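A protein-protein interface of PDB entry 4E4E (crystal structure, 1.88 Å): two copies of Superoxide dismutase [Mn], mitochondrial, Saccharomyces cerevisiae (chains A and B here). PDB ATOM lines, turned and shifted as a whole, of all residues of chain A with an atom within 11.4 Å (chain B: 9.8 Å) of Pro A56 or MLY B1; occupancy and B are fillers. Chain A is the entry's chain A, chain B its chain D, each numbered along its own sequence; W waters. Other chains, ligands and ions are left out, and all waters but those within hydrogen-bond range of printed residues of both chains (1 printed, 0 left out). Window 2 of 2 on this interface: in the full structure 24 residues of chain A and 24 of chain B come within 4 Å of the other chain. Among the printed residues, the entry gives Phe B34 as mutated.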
ATOM      1  N   PHE A  45      20.861  -3.590  15.660  1.00  0.00           N
ATOM      2  CA  PHE A  45      21.579  -4.646  16.355  1.00  0.00           C
ATOM      3  C   PHE A  45      21.314  -4.608  17.856  1.00  0.00           C
ATOM      4  O   PHE A  45      21.241  -5.657  18.487  1.00  0.00           O
ATOM      5  CB  PHE A  45      23.080  -4.659  16.060  1.00  0.00           C
ATOM      6  CG  PHE A  45      23.709  -6.002  16.298  1.00  0.00           C
ATOM      7  CD1 PHE A  45      23.782  -6.944  15.283  1.00  0.00           C
ATOM      8  CD2 PHE A  45      24.173  -6.347  17.553  1.00  0.00           C
ATOM      9  CE1 PHE A  45      24.326  -8.205  15.536  1.00  0.00           C
ATOM     10  CE2 PHE A  45      24.733  -7.586  17.808  1.00  0.00           C
ATOM     11  CZ  PHE A  45      24.818  -8.518  16.790  1.00  0.00           C
ATOM     12  N   GLU A  47      18.423  -3.715  19.144  1.00  0.00           N
ATOM     13  CA  GLU A  47      17.088  -4.320  19.211  1.00  0.00           C
ATOM     14  C   GLU A  47      17.148  -5.852  19.138  1.00  0.00           C
ATOM     15  O   GLU A  47      16.557  -6.564  19.976  1.00  0.00           O
ATOM     16  CB  GLU A  47      16.196  -3.756  18.096  1.00  0.00           C
ATOM     17  CG  GLU A  47      14.753  -4.283  18.101  1.00  0.00           C
ATOM     18  CD  GLU A  47      13.807  -3.425  17.257  1.00  0.00           C
ATOM     19  OE1 GLU A  47      13.426  -3.861  16.145  1.00  0.00           O
ATOM     20  OE2 GLU A  47      13.432  -2.316  17.711  1.00  0.00           O
ATOM     21  N   LEU A  48      17.876  -6.358  18.143  1.00  0.00           N
ATOM     22  CA  LEU A  48      18.010  -7.804  17.966  1.00  0.00           C
ATOM     23  C   LEU A  48      18.792  -8.452  19.088  1.00  0.00           C
ATOM     24  O   LEU A  48      18.628  -9.640  19.359  1.00  0.00           O
ATOM     25  CB  LEU A  48      18.676  -8.139  16.635  1.00  0.00           C
ATOM     26  CG  LEU A  48      17.837  -7.828  15.402  1.00  0.00           C
ATOM     27  CD1 LEU A  48      18.684  -8.042  14.168  1.00  0.00           C
ATOM     28  CD2 LEU A  48      16.595  -8.701  15.344  1.00  0.00           C
ATOM     29  N   SER A  49      19.647  -7.673  19.735  1.00  0.00           N
ATOM     30  CA  SER A  49      20.423  -8.160  20.863  1.00  0.00           C
ATOM     31  C   SER A  49      19.470  -8.442  22.018  1.00  0.00           C
ATOM     32  O   SER A  49      19.519  -9.525  22.646  1.00  0.00           O
ATOM     33  CB  SER A  49      21.473  -7.127  21.273  1.00  0.00           C
ATOM     34  OG  SER A  49      22.099  -7.515  22.483  1.00  0.00           O
ATOM     35  N   ASP A  50      18.584  -7.486  22.289  1.00  0.00           N
ATOM     36  CA  ASP A  50      17.563  -7.758  23.313  1.00  0.00           C
ATOM     37  C   ASP A  50      16.630  -8.927  22.938  1.00  0.00           C
ATOM     38  O   ASP A  50      16.288  -9.780  23.789  1.00  0.00           O
ATOM     39  CB  ASP A  50      16.757  -6.499  23.629  1.00  0.00           C
ATOM     40  CG  ASP A  50      17.364  -5.688  24.764  1.00  0.00           C
ATOM     41  OD1 ASP A  50      18.596  -5.788  24.994  1.00  0.00           O
ATOM     42  OD2 ASP A  50      16.598  -4.955  25.427  1.00  0.00           O
ATOM     43  N   LEU A  51      16.224  -8.966  21.668  1.00  0.00           N
ATOM     44  CA  LEU A  51      15.363 -10.056  21.198  1.00  0.00           C
ATOM     45  C   LEU A  51      16.012 -11.435  21.355  1.00  0.00           C
ATOM     46  O   LEU A  51      15.356 -12.418  21.724  1.00  0.00           O
ATOM     47  CB  LEU A  51      14.955  -9.816  19.743  1.00  0.00           C
ATOM     48  CG  LEU A  51      13.490  -9.430  19.490  1.00  0.00           C
ATOM     49  CD1 LEU A  51      12.885  -8.619  20.639  1.00  0.00           C
ATOM     50  CD2 LEU A  51      13.370  -8.664  18.184  1.00  0.00           C
ATOM     51  N   LEU A  52      17.310 -11.501  21.078  1.00  0.00           N
ATOM     52  CA  LEU A  52      18.074 -12.727  21.223  1.00  0.00           C
ATOM     53  C   LEU A  52      18.177 -13.091  22.694  1.00  0.00           C
ATOM     54  O   LEU A  52      18.059 -14.266  23.049  1.00  0.00           O
ATOM     55  CB  LEU A  52      19.473 -12.567  20.629  1.00  0.00           C
ATOM     56  CG  LEU A  52      20.279 -13.864  20.569  1.00  0.00           C
ATOM     57  CD1 LEU A  52      19.862 -14.697  19.370  1.00  0.00           C
ATOM     58  CD2 LEU A  52      21.771 -13.558  20.514  1.00  0.00           C
ATOM     59  N   ALA A  53      18.384 -12.093  23.554  1.00  0.00           N
ATOM     60  CA  ALA A  53      18.376 -12.359  25.000  1.00  0.00           C
ATOM     61  C   ALA A  53      17.074 -13.040  25.433  1.00  0.00           C
ATOM     62  O   ALA A  53      17.092 -14.097  26.113  1.00  0.00           O
ATOM     63  CB  ALA A  53      18.596 -11.070  25.787  1.00  0.00           C
ATOM     64  N   MLY A  54      15.948 -12.457  25.029  1.00  0.00           N
ATOM     65  CA  MLY A  54      14.645 -13.022  25.403  1.00  0.00           C
ATOM     66  CB  MLY A  54      13.527 -12.043  25.041  1.00  0.00           C
ATOM     67  CG  MLY A  54      13.607 -10.731  25.807  1.00  0.00           C
ATOM     68  CD  MLY A  54      12.518  -9.766  25.364  1.00  0.00           C
ATOM     69  CE  MLY A  54      12.885  -8.344  25.774  1.00  0.00           C
ATOM     70  NZ  MLY A  54      11.855  -7.288  25.526  1.00  0.00           N
ATOM     71  CH1 MLY A  54      10.771  -7.830  24.700  1.00  0.00           C
ATOM     72  CH2 MLY A  54      11.266  -6.953  26.828  1.00  0.00           C
ATOM     73  C   MLY A  54      14.359 -14.393  24.785  1.00  0.00           C
ATOM     74  O   MLY A  54      13.600 -15.182  25.336  1.00  0.00           O
ATOM     75  N   GLU A  55      14.996 -14.682  23.652  1.00  0.00           N
ATOM     76  CA  GLU A  55      14.654 -15.851  22.844  1.00  0.00           C
ATOM     77  C   GLU A  55      15.863 -16.209  21.972  1.00  0.00           C
ATOM     78  O   GLU A  55      15.936 -15.805  20.805  1.00  0.00           O
ATOM     79  CB  GLU A  55      13.474 -15.460  21.958  1.00  0.00           C
ATOM     80  CG  GLU A  55      12.841 -16.551  21.120  1.00  0.00           C
ATOM     81  CD  GLU A  55      11.595 -16.034  20.419  1.00  0.00           C
ATOM     82  OE1 GLU A  55      11.732 -15.358  19.371  1.00  0.00           O
ATOM     83  OE2 GLU A  55      10.480 -16.278  20.933  1.00  0.00           O
ATOM     84  N   PRO A  56      16.837 -16.940  22.540  1.00  0.00           N
ATOM     85  CA  PRO A  56      18.128 -17.160  21.863  1.00  0.00           C
ATOM     86  C   PRO A  56      18.084 -18.318  20.867  1.00  0.00           C
ATOM     87  O   PRO A  56      18.784 -19.331  21.031  1.00  0.00           O
ATOM     88  CB  PRO A  56      19.083 -17.471  23.028  1.00  0.00           C
ATOM     89  CG  PRO A  56      18.196 -18.118  24.062  1.00  0.00           C
ATOM     90  CD  PRO A  56      16.851 -17.416  23.935  1.00  0.00           C
ATOM     91  N   SER A  57      17.268 -18.159  19.831  1.00  0.00           N
ATOM     92  CA  SER A  57      17.063 -19.217  18.850  1.00  0.00           C
ATOM     93  C   SER A  57      17.983 -19.012  17.653  1.00  0.00           C
ATOM     94  O   SER A  57      18.510 -17.915  17.442  1.00  0.00           O
ATOM     95  CB  SER A  57      15.619 -19.191  18.363  1.00  0.00           C
ATOM     96  OG  SER A  57      15.379 -17.996  17.633  1.00  0.00           O
ATOM     97  N   PRO A  58      18.167 -20.067  16.849  1.00  0.00           N
ATOM     98  CA  PRO A  58      18.858 -19.913  15.564  1.00  0.00           C
ATOM     99  C   PRO A  58      18.188 -18.889  14.630  1.00  0.00           C
ATOM    100  O   PRO A  58      18.885 -18.246  13.849  1.00  0.00           O
ATOM    101  CB  PRO A  58      18.765 -21.312  14.948  1.00  0.00           C
ATOM    102  CG  PRO A  58      18.678 -22.236  16.114  1.00  0.00           C
ATOM    103  CD  PRO A  58      17.935 -21.485  17.197  1.00  0.00           C
ATOM    104  N   ALA A  59      16.862 -18.742  14.687  1.00  0.00           N
ATOM    105  CA  ALA A  59      16.190 -17.748  13.833  1.00  0.00           C
ATOM    106  C   ALA A  59      16.659 -16.308  14.106  1.00  0.00           C
ATOM    107  O   ALA A  59      17.013 -15.530  13.181  1.00  0.00           O
ATOM    108  CB  ALA A  59      14.673 -17.861  13.979  1.00  0.00           C
ATOM    109  N   ASN A  60      16.666 -15.948  15.384  1.00  0.00           N
ATOM    110  CA  ASN A  60      17.112 -14.620  15.784  1.00  0.00           C
ATOM    111  C   ASN A  60      18.611 -14.390  15.498  1.00  0.00           C
ATOM    112  O   ASN A  60      19.042 -13.301  15.046  1.00  0.00           O
ATOM    113  CB  ASN A  60      16.722 -14.369  17.252  1.00  0.00           C
ATOM    114  CG  ASN A  60      15.213 -14.233  17.429  1.00  0.00           C
ATOM    115  OD1 ASN A  60      14.495 -13.909  16.475  1.00  0.00           O
ATOM    116  ND2 ASN A  60      14.722 -14.484  18.644  1.00  0.00           N
ATOM    117  N   ALA A  61      19.402 -15.435  15.725  1.00  0.00           N
ATOM    118  CA  ALA A  61      20.824 -15.374  15.389  1.00  0.00           C
ATOM    119  C   ALA A  61      21.005 -15.098  13.889  1.00  0.00           C
ATOM    120  O   ALA A  61      21.853 -14.291  13.478  1.00  0.00           O
ATOM    121  CB  ALA A  61      21.512 -16.662  15.797  1.00  0.00           C
ATOM    122  N   ARG A  62      20.178 -15.764  13.083  1.00  0.00           N
ATOM    123  CA  ARG A  62      20.150 -15.586  11.631  1.00  0.00           C
ATOM    124  C   ARG A  62      19.867 -14.122  11.272  1.00  0.00           C
ATOM    125  O   ARG A  62      20.533 -13.526  10.385  1.00  0.00           O
ATOM    126  CB  ARG A  62      19.074 -16.512  11.045  1.00  0.00           C
ATOM    127  CG  ARG A  62      19.134 -16.737   9.539  1.00  0.00           C
ATOM    128  CD  ARG A  62      18.147 -17.841   9.113  1.00  0.00           C
ATOM    129  NE  ARG A  62      17.795 -17.730   7.699  1.00  0.00           N
ATOM    130  CZ  ARG A  62      16.652 -17.210   7.259  1.00  0.00           C
ATOM    131  NH1 ARG A  62      15.744 -16.781   8.135  1.00  0.00           N
ATOM    132  NH2 ARG A  62      16.409 -17.126   5.953  1.00  0.00           N
ATOM    133  N   MLY A  63      18.891 -13.533  11.968  1.00  0.00           N
ATOM    134  CA  MLY A  63      18.610 -12.100  11.762  1.00  0.00           C
ATOM    135  CB  MLY A  63      17.381 -11.689  12.573  1.00  0.00           C
ATOM    136  CG  MLY A  63      16.091 -12.311  12.062  1.00  0.00           C
ATOM    137  CD  MLY A  63      14.930 -11.842  12.916  1.00  0.00           C
ATOM    138  CE  MLY A  63      13.597 -12.391  12.421  1.00  0.00           C
ATOM    139  NZ  MLY A  63      12.629 -12.538  13.550  1.00  0.00           N
ATOM    140  CH1 MLY A  63      12.844 -11.454  14.523  1.00  0.00           C
ATOM    141  CH2 MLY A  63      11.275 -12.357  13.016  1.00  0.00           C
ATOM    142  C   MLY A  63      19.807 -11.169  12.069  1.00  0.00           C
ATOM    143  O   MLY A  63      20.119 -10.213  11.297  1.00  0.00           O
ATOM    144  N   MET A  64      20.500 -11.465  13.174  1.00  0.00           N
ATOM    145  CA  MET A  64      21.710 -10.693  13.506  1.00  0.00           C
ATOM    146  C   MET A  64      22.811 -10.818  12.446  1.00  0.00           C
ATOM    147  O   MET A  64      23.467  -9.816  12.074  1.00  0.00           O
ATOM    148  CB  MET A  64      22.247 -11.082  14.880  1.00  0.00           C
ATOM    149  CG  MET A  64      21.306 -10.695  15.999  1.00  0.00           C
ATOM    150  SD  MET A  64      21.592 -11.653  17.500  1.00  0.00           S
ATOM    151  CE  MET A  64      22.854 -10.681  18.324  1.00  0.00           C
ATOM    152  N   MLY B   1      22.080 -15.057  25.396  1.00  0.00           N
ATOM    153  CA  MLY B   1      23.004 -16.178  25.562  1.00  0.00           C
ATOM    154  CB  MLY B   1      23.279 -16.454  27.045  1.00  0.00           C
ATOM    155  CG  MLY B   1      24.126 -17.704  27.264  1.00  0.00           C
ATOM    156  CD  MLY B   1      24.533 -17.869  28.722  1.00  0.00           C
ATOM    157  CE  MLY B   1      25.253 -19.195  28.937  1.00  0.00           C
ATOM    158  NZ  MLY B   1      25.776 -19.345  30.332  1.00  0.00           N
ATOM    159  CH1 MLY B   1      24.838 -20.221  31.056  1.00  0.00           C
ATOM    160  CH2 MLY B   1      27.063 -20.055  30.253  1.00  0.00           C
ATOM    161  C   MLY B   1      22.515 -17.467  24.902  1.00  0.00           C
ATOM    162  O   MLY B   1      21.555 -18.092  25.365  1.00  0.00           O
ATOM    163  N   VAL B   2      23.208 -17.886  23.845  1.00  0.00           N
ATOM    164  CA  VAL B   2      22.848 -19.116  23.158  1.00  0.00           C
ATOM    165  C   VAL B   2      23.459 -20.335  23.863  1.00  0.00           C
ATOM    166  O   VAL B   2      24.435 -20.222  24.626  1.00  0.00           O
ATOM    167  CB  VAL B   2      23.208 -19.088  21.637  1.00  0.00           C
ATOM    168  CG1 VAL B   2      22.533 -17.893  20.934  1.00  0.00           C
ATOM    169  CG2 VAL B   2      24.717 -19.014  21.420  1.00  0.00           C
ATOM    170  N   THR B   3      22.869 -21.494  23.606  1.00  0.00           N
ATOM    171  CA  THR B   3      23.311 -22.757  24.202  1.00  0.00           C
ATOM    172  C   THR B   3      23.280 -23.855  23.136  1.00  0.00           C
ATOM    173  O   THR B   3      22.483 -23.763  22.200  1.00  0.00           O
ATOM    174  CB  THR B   3      22.364 -23.170  25.360  1.00  0.00           C
ATOM    175  OG1 THR B   3      22.112 -22.042  26.210  1.00  0.00           O
ATOM    176  CG2 THR B   3      22.982 -24.289  26.188  1.00  0.00           C
ATOM    177  N   LEU B   4      24.136 -24.877  23.262  1.00  0.00           N
ATOM    178  CA  LEU B   4      24.033 -26.064  22.412  1.00  0.00           C
ATOM    179  C   LEU B   4      22.606 -26.601  22.480  1.00  0.00           C
ATOM    180  O   LEU B   4      22.039 -26.748  23.571  1.00  0.00           O
ATOM    181  CB  LEU B   4      24.973 -27.181  22.872  1.00  0.00           C
ATOM    182  CG  LEU B   4      26.418 -27.322  22.407  1.00  0.00           C
ATOM    183  CD1 LEU B   4      26.925 -28.702  22.833  1.00  0.00           C
ATOM    184  CD2 LEU B   4      26.564 -27.130  20.905  1.00  0.00           C
ATOM    185  N   PRO B   5      22.026 -26.913  21.315  1.00  0.00           N
ATOM    186  CA  PRO B   5      20.686 -27.506  21.330  1.00  0.00           C
ATOM    187  C   PRO B   5      20.780 -28.949  21.817  1.00  0.00           C
ATOM    188  O   PRO B   5      21.849 -29.564  21.688  1.00  0.00           O
ATOM    189  CB  PRO B   5      20.290 -27.489  19.852  1.00  0.00           C
ATOM    190  CG  PRO B   5      21.632 -27.647  19.116  1.00  0.00           C
ATOM    191  CD  PRO B   5      22.600 -26.841  19.955  1.00  0.00           C
ATOM    192  N   HIS B  31      30.590 -27.379  17.578  1.00  0.00           N
ATOM    193  CA  HIS B  31      29.371 -26.601  17.746  1.00  0.00           C
ATOM    194  C   HIS B  31      29.449 -25.769  19.024  1.00  0.00           C
ATOM    195  O   HIS B  31      29.082 -24.587  19.041  1.00  0.00           O
ATOM    196  CB  HIS B  31      28.133 -27.501  17.710  1.00  0.00           C
ATOM    197  CG  HIS B  31      26.865 -26.753  17.488  1.00  0.00           C
ATOM    198  ND1 HIS B  31      25.631 -27.377  17.414  1.00  0.00           N
ATOM    199  CD2 HIS B  31      26.613 -25.433  17.311  1.00  0.00           C
ATOM    200  CE1 HIS B  31      24.690 -26.484  17.211  1.00  0.00           C
ATOM    201  NE2 HIS B  31      25.268 -25.281  17.145  1.00  0.00           N
ATOM    202  N   GLN B  32      29.984 -26.376  20.077  1.00  0.00           N
ATOM    203  CA  GLN B  32      30.107 -25.699  21.364  1.00  0.00           C
ATOM    204  C   GLN B  32      31.038 -24.491  21.241  1.00  0.00           C
ATOM    205  O   GLN B  32      30.860 -23.456  21.924  1.00  0.00           O
ATOM    206  CB  GLN B  32      30.618 -26.677  22.427  1.00  0.00           C
ATOM    207  CG  GLN B  32      30.798 -26.037  23.785  1.00  0.00           C
ATOM    208  CD  GLN B  32      29.469 -25.708  24.421  1.00  0.00           C
ATOM    209  OE1 GLN B  32      28.714 -26.603  24.774  1.00  0.00           O
ATOM    210  NE2 GLN B  32      29.173 -24.423  24.556  1.00  0.00           N
ATOM    211  N   PHE B  34      31.408 -22.688  18.478  1.00  0.00           N
ATOM    212  CA  PHE B  34      30.607 -21.597  17.887  1.00  0.00           C
ATOM    213  C   PHE B  34      29.632 -20.973  18.900  1.00  0.00           C
ATOM    214  O   PHE B  34      29.386 -19.776  18.846  1.00  0.00           O
ATOM    215  CB  PHE B  34      29.831 -22.070  16.657  1.00  0.00           C
ATOM    216  CG  PHE B  34      30.700 -22.391  15.473  1.00  0.00           C
ATOM    217  CD1 PHE B  34      31.559 -21.435  14.943  1.00  0.00           C
ATOM    218  CD2 PHE B  34      30.647 -23.645  14.883  1.00  0.00           C
ATOM    219  CE1 PHE B  34      32.360 -21.736  13.843  1.00  0.00           C
ATOM    220  CE2 PHE B  34      31.442 -23.944  13.788  1.00  0.00           C
ATOM    221  CZ  PHE B  34      32.288 -22.978  13.265  1.00  0.00           C
ATOM    222  N   VAL B  35      29.069 -21.777  19.798  1.00  0.00           N
ATOM    223  CA  VAL B  35      28.176 -21.244  20.845  1.00  0.00           C
ATOM    224  C   VAL B  35      28.934 -20.192  21.673  1.00  0.00           C
ATOM    225  O   VAL B  35      28.500 -19.015  21.813  1.00  0.00           O
ATOM    226  CB  VAL B  35      27.638 -22.382  21.753  1.00  0.00           C
ATOM    227  CG1 VAL B  35      26.931 -21.830  23.009  1.00  0.00           C
ATOM    228  CG2 VAL B  35      26.694 -23.315  20.958  1.00  0.00           C
ATOM    229  N   ASN B  36      30.090 -20.615  22.187  1.00  0.00           N
ATOM    230  CA  ASN B  36      30.934 -19.742  23.007  1.00  0.00           C
ATOM    231  C   ASN B  36      31.371 -18.492  22.258  1.00  0.00           C
ATOM    232  O   ASN B  36      31.286 -17.368  22.769  1.00  0.00           O
ATOM    233  CB  ASN B  36      32.158 -20.515  23.519  1.00  0.00           C
ATOM    234  CG  ASN B  36      31.783 -21.667  24.434  1.00  0.00           C
ATOM    235  OD1 ASN B  36      30.649 -21.750  24.920  1.00  0.00           O
ATOM    236  ND2 ASN B  36      32.739 -22.564  24.683  1.00  0.00           N
ATOM    237  N   PHE B  38      29.999 -17.084  19.650  1.00  0.00           N
ATOM    238  CA  PHE B  38      28.895 -16.198  19.317  1.00  0.00           C
ATOM    239  C   PHE B  38      28.535 -15.360  20.542  1.00  0.00           C
ATOM    240  O   PHE B  38      28.346 -14.129  20.438  1.00  0.00           O
ATOM    241  CB  PHE B  38      27.687 -16.995  18.820  1.00  0.00           C
ATOM    242  CG  PHE B  38      26.568 -16.135  18.302  1.00  0.00           C
ATOM    243  CD1 PHE B  38      26.817 -15.139  17.373  1.00  0.00           C
ATOM    244  CD2 PHE B  38      25.262 -16.331  18.728  1.00  0.00           C
ATOM    245  CE1 PHE B  38      25.788 -14.348  16.881  1.00  0.00           C
ATOM    246  CE2 PHE B  38      24.229 -15.527  18.242  1.00  0.00           C
ATOM    247  CZ  PHE B  38      24.495 -14.545  17.317  1.00  0.00           C
ATOM    248  N   ASN B  39      28.477 -16.020  21.702  1.00  0.00           N
ATOM    249  CA  ASN B  39      28.148 -15.298  22.937  1.00  0.00           C
ATOM    250  C   ASN B  39      29.180 -14.214  23.248  1.00  0.00           C
ATOM    251  O   ASN B  39      28.828 -13.055  23.577  1.00  0.00           O
ATOM    252  CB  ASN B  39      27.979 -16.274  24.118  1.00  0.00           C
ATOM    253  CG  ASN B  39      26.707 -17.104  24.003  1.00  0.00           C
ATOM    254  OD1 ASN B  39      25.708 -16.638  23.448  1.00  0.00           O
ATOM    255  ND2 ASN B  39      26.735 -18.333  24.527  1.00  0.00           N
ATOM    256  N   THR B  40      30.455 -14.578  23.103  1.00  0.00           N
ATOM    257  CA  THR B  40      31.528 -13.618  23.314  1.00  0.00           C
ATOM    258  C   THR B  40      31.421 -12.450  22.329  1.00  0.00           C
ATOM    259  O   THR B  40      31.583 -11.286  22.717  1.00  0.00           O
ATOM    260  CB  THR B  40      32.920 -14.286  23.195  1.00  0.00           C
ATOM    261  OG1 THR B  40      33.038 -15.309  24.197  1.00  0.00           O
ATOM    262  CG2 THR B  40      34.016 -13.268  23.403  1.00  0.00           C
ATOM    263  N   VAL B  42      28.769 -11.232  20.783  1.00  0.00           N
ATOM    264  CA  VAL B  42      27.642 -10.352  21.095  1.00  0.00           C
ATOM    265  C   VAL B  42      27.896  -9.504  22.354  1.00  0.00           C
ATOM    266  O   VAL B  42      27.540  -8.310  22.387  1.00  0.00           O
ATOM    267  CB  VAL B  42      26.297 -11.116  21.154  1.00  0.00           C
ATOM    268  CG1 VAL B  42      25.155 -10.173  21.545  1.00  0.00           C
ATOM    269  CG2 VAL B  42      26.002 -11.722  19.793  1.00  0.00           C
ATOM    270  N   ASP B  43      28.537 -10.094  23.368  1.00  0.00           N
ATOM    271  CA  ASP B  43      28.967  -9.284  24.520  1.00  0.00           C
ATOM    272  C   ASP B  43      29.910  -8.139  24.101  1.00  0.00           C
ATOM    273  O   ASP B  43      29.688  -6.953  24.454  1.00  0.00           O
ATOM    274  CB  ASP B  43      29.635 -10.155  25.596  1.00  0.00           C
ATOM    275  CG  ASP B  43      28.661 -11.136  26.249  1.00  0.00           C
ATOM    276  OD1 ASP B  43      27.428 -10.894  26.193  1.00  0.00           O
ATOM    277  OD2 ASP B  43      29.132 -12.146  26.828  1.00  0.00           O
ATOM    278  N   PHE B  78      26.879 -21.381  14.634  1.00  0.00           N
ATOM    279  CA  PHE B  78      25.827 -21.777  15.570  1.00  0.00           C
ATOM    280  C   PHE B  78      24.538 -22.169  14.823  1.00  0.00           C
ATOM    281  O   PHE B  78      24.014 -23.297  14.975  1.00  0.00           O
ATOM    282  CB  PHE B  78      25.563 -20.651  16.574  1.00  0.00           C
ATOM    283  CG  PHE B  78      24.365 -20.896  17.447  1.00  0.00           C
ATOM    284  CD1 PHE B  78      24.387 -21.906  18.398  1.00  0.00           C
ATOM    285  CD2 PHE B  78      23.216 -20.131  17.304  1.00  0.00           C
ATOM    286  CE1 PHE B  78      23.273 -22.145  19.212  1.00  0.00           C
ATOM    287  CE2 PHE B  78      22.101 -20.357  18.106  1.00  0.00           C
ATOM    288  CZ  PHE B  78      22.130 -21.364  19.059  1.00  0.00           C
ATOM    289  N   THR B  79      24.056 -21.244  13.988  1.00  0.00           N
ATOM    290  CA  THR B  79      22.798 -21.465  13.260  1.00  0.00           C
ATOM    291  C   THR B  79      22.854 -22.656  12.303  1.00  0.00           C
ATOM    292  O   THR B  79      21.938 -23.501  12.279  1.00  0.00           O
ATOM    293  CB  THR B  79      22.348 -20.183  12.503  1.00  0.00           C
ATOM    294  OG1 THR B  79      23.234 -19.913  11.419  1.00  0.00           O
ATOM    295  CG2 THR B  79      22.377 -18.999  13.429  1.00  0.00           C
ATOM    296  N   CYS B  82      22.768 -25.911  14.201  1.00  0.00           N
ATOM    297  CA  CYS B  82      21.415 -26.215  14.709  1.00  0.00           C
ATOM    298  C   CYS B  82      20.515 -26.810  13.611  1.00  0.00           C
ATOM    299  O   CYS B  82      19.864 -27.888  13.789  1.00  0.00           O
ATOM    300  CB  CYS B  82      20.759 -24.977  15.302  1.00  0.00           C
ATOM    301  SG  CYS B  82      21.455 -24.424  16.872  1.00  0.00           S
HETATM  302  O   HOH W   1      20.263 -21.197  22.568  1.00  0.00           O
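SG of Cys B82 is in hydrogen-bond range of O of Phe B78.
Phe B38 touches Leu A52.
Pro A56 touches MLY B1.
Pro A58 touches Thr B79.
CG of Pro A58 touches CB of Cys B82 (3.5 Å).
CB of Ala A61 touches CE2 of Phe B38, 3.8 Å away.
Thr B79 touches Ala A61 (CG2 to CB, 3.4 Å).
Thr B79 touches Arg A62.
Val B42 touches Met A64 (CG2 to CE, 3.6 Å).
Printed residues of chain B within 4 Å of Pro A56: MLY B1.
No residue of chain B comes within 4 Å of Ser A57.
Printed residues of chain B within 4 Å of Pro A58: Thr B79 (3.6 Å) and Cys B82 (3.5 Å).
Of the printed residues of chain B, Met A64 touches Val B42.
MLY B1 touches just one residue of chain A: Pro A56.
No residue of chain A comes within 4 Å of Thr B3.
No residue of chain A comes within 4 Å of Asn B39.
Asp B43 touches none of the printed residues of chain A.
Printed residues of chain B that touch a printed residue of chain A: MLY B1, Phe B38, Val B42, Thr B79 and Cys B82.
Of the 19 printed residues of chain A, 6 touch a printed residue of chain B.
Printed residues of chain A that touch a printed residue of chain B: Leu A52, Pro A56, Pro A58, Ala A61, Arg A62 and Met A64.
Hydrophobic or aromatic side chains of chain A within 4 Å of the printed part of chain B: Leu A52, Pro A56, Pro A58, Ala A61 and Met A64.
Along chain A the printed residues that touch a printed residue of chain B span positions 52 to 64.
Among the printed residues, no Asp or Glu carboxylate lies within 4 Å of a Lys or Arg side-chain nitrogen of the other chain.
No position is printed for both chains.
Water W1 bridges the backbone NH (N) of Thr B3 (2.8 Å) and the backbone carbonyl oxygen (O) of Pro A56 (2.8 Å).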
